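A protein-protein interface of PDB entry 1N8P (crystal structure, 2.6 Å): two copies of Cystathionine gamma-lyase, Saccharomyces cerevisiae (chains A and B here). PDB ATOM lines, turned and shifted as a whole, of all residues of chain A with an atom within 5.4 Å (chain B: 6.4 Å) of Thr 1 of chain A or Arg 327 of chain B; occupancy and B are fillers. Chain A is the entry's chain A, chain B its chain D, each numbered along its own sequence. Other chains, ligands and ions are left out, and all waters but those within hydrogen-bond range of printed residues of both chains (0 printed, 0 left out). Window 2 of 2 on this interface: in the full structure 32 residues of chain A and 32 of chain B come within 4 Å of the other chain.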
ATOM      1  N   THR A   1      -4.722  14.445  11.115  1.00  0.00           N
ATOM      2  CA  THR A   1      -5.560  13.366  11.713  1.00  0.00           C
ATOM      3  C   THR A   1      -7.044  13.700  11.569  1.00  0.00           C
ATOM      4  O   THR A   1      -7.435  14.880  11.541  1.00  0.00           O
ATOM      5  CB  THR A   1      -5.225  13.143  13.251  1.00  0.00           C
ATOM      6  OG1 THR A   1      -4.433  11.961  13.418  1.00  0.00           O
ATOM      7  CG2 THR A   1      -6.486  12.963  14.066  1.00  0.00           C
ATOM      8  N   LEU A   2      -7.853  12.645  11.469  1.00  0.00           N
ATOM      9  CA  LEU A   2      -9.299  12.773  11.376  1.00  0.00           C
ATOM     10  C   LEU A   2      -9.950  11.505  11.932  1.00  0.00           C
ATOM     11  O   LEU A   2     -10.074  10.492  11.231  1.00  0.00           O
ATOM     12  CB  LEU A   2      -9.746  13.006   9.931  1.00  0.00           C
ATOM     13  CG  LEU A   2     -11.270  13.155   9.810  1.00  0.00           C
ATOM     14  CD1 LEU A   2     -11.625  14.325   8.893  1.00  0.00           C
ATOM     15  CD2 LEU A   2     -11.879  11.832   9.326  1.00  0.00           C
ATOM     16  N   GLN A   3     -10.363  11.571  13.197  1.00  0.00           N
ATOM     17  CA  GLN A   3     -10.995  10.441  13.870  1.00  0.00           C
ATOM     18  C   GLN A   3     -12.129   9.850  13.064  1.00  0.00           C
ATOM     19  O   GLN A   3     -12.822  10.554  12.339  1.00  0.00           O
ATOM     20  CB  GLN A   3     -11.541  10.873  15.224  1.00  0.00           C
ATOM     21  CG  GLN A   3     -10.502  11.296  16.218  1.00  0.00           C
ATOM     22  CD  GLN A   3     -11.054  12.360  17.122  1.00  0.00           C
ATOM     23  OE1 GLN A   3     -11.217  13.512  16.710  1.00  0.00           O
ATOM     24  NE2 GLN A   3     -11.379  11.981  18.358  1.00  0.00           N
ATOM     25  N   GLU A   4     -12.326   8.549  13.226  1.00  0.00           N
ATOM     26  CA  GLU A   4     -13.364   7.833  12.512  1.00  0.00           C
ATOM     27  C   GLU A   4     -13.805   6.628  13.341  1.00  0.00           C
ATOM     28  O   GLU A   4     -13.668   5.474  12.909  1.00  0.00           O
ATOM     29  CB  GLU A   4     -12.818   7.388  11.152  1.00  0.00           C
ATOM     30  CG  GLU A   4     -12.206   8.546  10.341  1.00  0.00           C
ATOM     31  CD  GLU A   4     -11.580   8.100   9.036  1.00  0.00           C
ATOM     32  OE1 GLU A   4     -10.900   7.051   9.043  1.00  0.00           O
ATOM     33  OE2 GLU A   4     -11.751   8.805   8.015  1.00  0.00           O
ATOM     34  N   ASP A   6     -12.537   5.661  16.220  1.00  0.00           N
ATOM     35  CA  ASP A   6     -11.313   5.054  16.709  1.00  0.00           C
ATOM     36  C   ASP A   6     -11.479   4.812  18.211  1.00  0.00           C
ATOM     37  O   ASP A   6     -12.540   5.084  18.778  1.00  0.00           O
ATOM     38  CB  ASP A   6     -10.159   6.009  16.458  1.00  0.00           C
ATOM     39  CG  ASP A   6      -9.955   6.282  14.989  1.00  0.00           C
ATOM     40  OD1 ASP A   6      -9.481   5.379  14.291  1.00  0.00           O
ATOM     41  OD2 ASP A   6     -10.275   7.384  14.516  1.00  0.00           O
ATOM     42  N   HIS A  14      -6.620  13.353  19.617  1.00  0.00           N
ATOM     43  CA  HIS A  14      -6.979  14.135  18.432  1.00  0.00           C
ATOM     44  C   HIS A  14      -8.289  14.875  18.448  1.00  0.00           C
ATOM     45  O   HIS A  14      -8.413  15.911  17.793  1.00  0.00           O
ATOM     46  CB  HIS A  14      -6.916  13.224  17.216  1.00  0.00           C
ATOM     47  CG  HIS A  14      -5.563  12.625  16.990  1.00  0.00           C
ATOM     48  ND1 HIS A  14      -4.476  13.379  16.610  1.00  0.00           N
ATOM     49  CD2 HIS A  14      -5.118  11.357  17.110  1.00  0.00           C
ATOM     50  CE1 HIS A  14      -3.417  12.597  16.503  1.00  0.00           C
ATOM     51  NE2 HIS A  14      -3.780  11.363  16.798  1.00  0.00           N
ATOM     52  N   GLU A  17      -8.947  18.910  17.876  1.00  0.00           N
ATOM     53  CA  GLU A  17      -7.867  19.528  17.114  1.00  0.00           C
ATOM     54  C   GLU A  17      -8.238  20.970  16.789  1.00  0.00           C
ATOM     55  O   GLU A  17      -9.420  21.319  16.769  1.00  0.00           O
ATOM     56  CB  GLU A  17      -7.618  18.762  15.819  1.00  0.00           C
ATOM     57  CG  GLU A  17      -6.325  19.155  15.149  1.00  0.00           C
ATOM     58  CD  GLU A  17      -6.071  18.382  13.875  1.00  0.00           C
ATOM     59  OE1 GLU A  17      -4.894  18.355  13.434  1.00  0.00           O
ATOM     60  OE2 GLU A  17      -7.048  17.814  13.319  1.00  0.00           O
ATOM     61  N   SER B 324       1.770  10.514   3.716  1.00  0.00           N
ATOM     62  CA  SER B 324       0.548  11.292   3.578  1.00  0.00           C
ATOM     63  C   SER B 324      -0.726  10.460   3.704  1.00  0.00           C
ATOM     64  O   SER B 324      -1.639  10.828   4.449  1.00  0.00           O
ATOM     65  CB  SER B 324       0.575  12.021   2.228  1.00  0.00           C
ATOM     66  OG  SER B 324       1.818  12.693   2.033  1.00  0.00           O
ATOM     67  N   SER B 325      -0.802   9.354   2.965  1.00  0.00           N
ATOM     68  CA  SER B 325      -1.977   8.470   3.028  1.00  0.00           C
ATOM     69  C   SER B 325      -2.410   8.258   4.490  1.00  0.00           C
ATOM     70  O   SER B 325      -3.609   8.207   4.796  1.00  0.00           O
ATOM     71  CB  SER B 325      -1.660   7.101   2.411  1.00  0.00           C
ATOM     72  OG  SER B 325      -1.208   7.214   1.072  1.00  0.00           O
ATOM     73  N   THR B 326      -1.417   8.123   5.379  1.00  0.00           N
ATOM     74  CA  THR B 326      -1.632   7.931   6.817  1.00  0.00           C
ATOM     75  C   THR B 326      -2.713   8.858   7.319  1.00  0.00           C
ATOM     76  O   THR B 326      -2.881   9.968   6.794  1.00  0.00           O
ATOM     77  CB  THR B 326      -0.390   8.278   7.620  1.00  0.00           C
ATOM     78  OG1 THR B 326       0.002   9.625   7.311  1.00  0.00           O
ATOM     79  CG2 THR B 326       0.730   7.322   7.299  1.00  0.00           C
ATOM     80  N   ARG B 327      -3.427   8.400   8.346  1.00  0.00           N
ATOM     81  CA  ARG B 327      -4.501   9.185   8.962  1.00  0.00           C
ATOM     82  C   ARG B 327      -4.123   9.535  10.398  1.00  0.00           C
ATOM     83  O   ARG B 327      -4.399  10.624  10.888  1.00  0.00           O
ATOM     84  CB  ARG B 327      -5.799   8.384   8.965  1.00  0.00           C
ATOM     85  CG  ARG B 327      -6.977   9.136   9.532  1.00  0.00           C
ATOM     86  CD  ARG B 327      -8.267   8.365   9.309  1.00  0.00           C
ATOM     87  NE  ARG B 327      -8.353   7.158  10.122  1.00  0.00           N
ATOM     88  CZ  ARG B 327      -8.606   7.165  11.430  1.00  0.00           C
ATOM     89  NH1 ARG B 327      -8.802   8.313  12.073  1.00  0.00           N
ATOM     90  NH2 ARG B 327      -8.661   6.027  12.095  1.00  0.00           N
ATOM     91  N   LEU B 328      -3.466   8.596  11.059  1.00  0.00           N
ATOM     92  CA  LEU B 328      -3.072   8.787  12.433  1.00  0.00           C
ATOM     93  C   LEU B 328      -1.669   9.392  12.608  1.00  0.00           C
ATOM     94  O   LEU B 328      -1.482  10.255  13.475  1.00  0.00           O
ATOM     95  CB  LEU B 328      -3.229   7.455  13.169  1.00  0.00           C
ATOM     96  CG  LEU B 328      -4.694   6.997  13.216  1.00  0.00           C
ATOM     97  CD1 LEU B 328      -4.896   5.793  14.142  1.00  0.00           C
ATOM     98  CD2 LEU B 328      -5.542   8.145  13.701  1.00  0.00           C
ATOM     99  N   PHE B 329      -0.693   8.957  11.801  1.00  0.00           N
ATOM    100  CA  PHE B 329       0.687   9.503  11.854  1.00  0.00           C
ATOM    101  C   PHE B 329       0.737  10.795  11.058  1.00  0.00           C
ATOM    102  O   PHE B 329       0.440  10.815   9.870  1.00  0.00           O
ATOM    103  CB  PHE B 329       1.711   8.531  11.259  1.00  0.00           C
ATOM    104  CG  PHE B 329       1.911   7.277  12.082  1.00  0.00           C
ATOM    105  CD1 PHE B 329       0.874   6.382  12.274  1.00  0.00           C
ATOM    106  CD2 PHE B 329       3.118   7.028  12.710  1.00  0.00           C
ATOM    107  CE1 PHE B 329       1.032   5.283  13.067  1.00  0.00           C
ATOM    108  CE2 PHE B 329       3.277   5.919  13.507  1.00  0.00           C
ATOM    109  CZ  PHE B 329       2.232   5.047  13.685  1.00  0.00           C
ATOM    110  N   THR B 330       1.124  11.872  11.722  1.00  0.00           N
ATOM    111  CA  THR B 330       1.181  13.178  11.112  1.00  0.00           C
ATOM    112  C   THR B 330       2.551  13.558  10.561  1.00  0.00           C
ATOM    113  O   THR B 330       3.563  13.623  11.282  1.00  0.00           O
ATOM    114  CB  THR B 330       0.726  14.223  12.130  1.00  0.00           C
ATOM    115  OG1 THR B 330      -0.590  13.880  12.566  1.00  0.00           O
ATOM    116  CG2 THR B 330       0.732  15.623  11.534  1.00  0.00           C
ATOM    117  N   SER B 340       1.340  10.718  17.464  1.00  0.00           N
ATOM    118  CA  SER B 340       2.095   9.960  16.452  1.00  0.00           C
ATOM    119  C   SER B 340       2.447  10.790  15.218  1.00  0.00           C
ATOM    120  O   SER B 340       1.588  11.452  14.632  1.00  0.00           O
ATOM    121  CB  SER B 340       1.310   8.744  15.997  1.00  0.00           C
ATOM    122  OG  SER B 340       1.277   7.757  17.006  1.00  0.00           O
ATOM    123  N   GLU B 375      -1.673   7.116  20.928  1.00  0.00           N
ATOM    124  CA  GLU B 375      -3.045   6.776  20.554  1.00  0.00           C
ATOM    125  C   GLU B 375      -3.259   5.266  20.780  1.00  0.00           C
ATOM    126  O   GLU B 375      -2.397   4.577  21.359  1.00  0.00           O
ATOM    127  CB  GLU B 375      -3.306   7.107  19.086  1.00  0.00           C
ATOM    128  CG  GLU B 375      -2.928   8.528  18.648  1.00  0.00           C
ATOM    129  CD  GLU B 375      -1.476   8.597  18.346  1.00  0.00           C
ATOM    130  OE1 GLU B 375      -1.005   9.621  17.818  1.00  0.00           O
ATOM    131  OE2 GLU B 375      -0.796   7.597  18.642  1.00  0.00           O
ATOM    132  N   ASP B 379      -5.568   0.928  16.697  1.00  0.00           N
ATOM    133  CA  ASP B 379      -5.940   2.025  15.809  1.00  0.00           C
ATOM    134  C   ASP B 379      -4.700   2.423  14.992  1.00  0.00           C
ATOM    135  O   ASP B 379      -4.790   2.812  13.828  1.00  0.00           O
ATOM    136  CB  ASP B 379      -6.385   3.244  16.617  1.00  0.00           C
ATOM    137  CG  ASP B 379      -7.744   3.066  17.262  1.00  0.00           C
ATOM    138  OD1 ASP B 379      -8.163   1.907  17.465  1.00  0.00           O
ATOM    139  OD2 ASP B 379      -8.390   4.089  17.583  1.00  0.00           O
ATOM    140  N   ASP B 383      -3.648   1.358  10.998  1.00  0.00           N
ATOM    141  CA  ASP B 383      -3.421   2.490  10.113  1.00  0.00           C
ATOM    142  C   ASP B 383      -2.141   2.340   9.293  1.00  0.00           C
ATOM    143  O   ASP B 383      -2.084   2.770   8.149  1.00  0.00           O
ATOM    144  CB  ASP B 383      -3.346   3.791  10.905  1.00  0.00           C
ATOM    145  CG  ASP B 383      -3.094   4.981  10.014  1.00  0.00           C
ATOM    146  OD1 ASP B 383      -4.033   5.428   9.340  1.00  0.00           O
ATOM    147  OD2 ASP B 383      -1.951   5.467   9.962  1.00  0.00           O
ATOM    148  N   GLN B 386      -3.246  -0.102   6.332  1.00  0.00           N
ATOM    149  CA  GLN B 386      -4.072   0.663   5.423  1.00  0.00           C
ATOM    150  C   GLN B 386      -3.219   1.726   4.724  1.00  0.00           C
ATOM    151  O   GLN B 386      -3.692   2.407   3.819  1.00  0.00           O
ATOM    152  CB  GLN B 386      -5.184   1.333   6.231  1.00  0.00           C
ATOM    153  CG  GLN B 386      -6.000   2.383   5.505  1.00  0.00           C
ATOM    154  CD  GLN B 386      -5.306   3.720   5.430  1.00  0.00           C
ATOM    155  OE1 GLN B 386      -4.367   3.982   6.183  1.00  0.00           O
ATOM    156  NE2 GLN B 386      -5.775   4.589   4.526  1.00  0.00           N
ATOM    157  N   ALA B 387      -1.967   1.875   5.145  1.00  0.00           N
ATOM    158  CA  ALA B 387      -1.081   2.875   4.563  1.00  0.00           C
ATOM    159  C   ALA B 387      -0.080   2.267   3.588  1.00  0.00           C
ATOM    160  O   ALA B 387       0.332   2.915   2.626  1.00  0.00           O
ATOM    161  CB  ALA B 387      -0.343   3.623   5.673  1.00  0.00           C
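The side-chain hydroxyl (OG1) of Thr 1 of chain A sits at hydrogen-bond distance from the backbone carbonyl oxygen (O) of Leu 328 of chain B (3.4 Å).
O of Arg 327 of chain B lies within hydrogen-bond range of OG1 of Thr 1 of chain A (2.9 Å).
The side-chain carboxylate of Glu 4 of chain A lies within salt-bridge range of the guanidinium group of Arg 327 of chain B.
A ring nitrogen (NE2) of His 14 of chain A sits at hydrogen-bond distance from the side-chain carboxylate (OE1) of Glu 375 of chain B (3.4 Å).
The guanidinium group of Arg 327 of chain B is in hydrogen-bond range of the backbone carbonyl oxygen of Leu 2 of chain A (2.7 Å).
The side-chain carboxylate (OD1) of Asp 6 of chain A lies within salt-bridge range of the guanidinium group (NH2) of Arg 327 of chain B (2.4 Å).
The side-chain hydroxyl (OG1) of Thr 1 of chain A lies close to a ring nitrogen (ND1) of His 14 of chain A (3.5 Å).
N of Arg 327 of chain B lies within hydrogen-bond range of OD1 of Asp 383 of chain B (3.2 Å).
N of Ser 340 of chain B sits at hydrogen-bond distance from OE1 of Glu 375 of chain B, 2.6 Å away.
N of Glu 4 of chain A lies within hydrogen-bond range of OD2 of Asp 6 of chain A, 2.7 Å away.
Arg 327 of chain B touches Gln 3 of chain A (NH1 to CA, 3.5 Å).
Asp 6 of chain A touches Asp 379 of chain B (CB to OD2, 2.8 Å).
Thr 1 of chain A touches two residues of chain B.
Printed residues of chain B within 4 Å of Gln 3 of chain A: Arg 327.
Thr 326 of chain B touches none of the printed residues of chain A.
Arg 327 of chain B touches just these residues of chain A: Thr 1, Leu 2, Gln 3, Glu 4 and Asp 6.
Of the printed residues of chain A, Leu 328 of chain B touches Thr 1 (3.4 Å).
Of the printed residues of chain A, Glu 375 of chain B touches His 14.
Printed residues of chain A within 4 Å of Asp 379 of chain B: Asp 6 (2.8 Å).
The nearest residue of chain B that does not touch Thr 1 of chain A is Thr 330 of chain B (4.4 Å).
The nearest printed residue of chain A that does not touch Arg 327 of chain B is His 14 of chain A (6.0 Å).
Of the 13 printed residues of chain B, 4 touch a printed residue of chain A.
Printed residues of chain B that touch a printed residue of chain A: Arg 327, Leu 328, Glu 375 and Asp 379.
Hydrophobic or aromatic side chains of chain B that line the printed part of chain A: Leu 328.
Of the 7 printed residues of chain A, 6 touch a printed residue of chain B.
Printed residues of chain A that touch a printed residue of chain B: Thr 1, Leu 2, Gln 3, Glu 4, Asp 6 and His 14.
Hydrophobic or aromatic side chains of chain A that line the printed part of chain B: His 14.
Among the printed residues, Asp or Glu carboxylates within 4 Å of a Lys or Arg side-chain nitrogen of the other chain: Glu 4 of chain A with Arg 327 of chain B and Asp 6 of chain A with Arg 327 of chain B.
No position is printed for both chains.
Of the 8 pairs that touch across the chains among the printed residues, none has its exchanged pair printed and touching as well.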
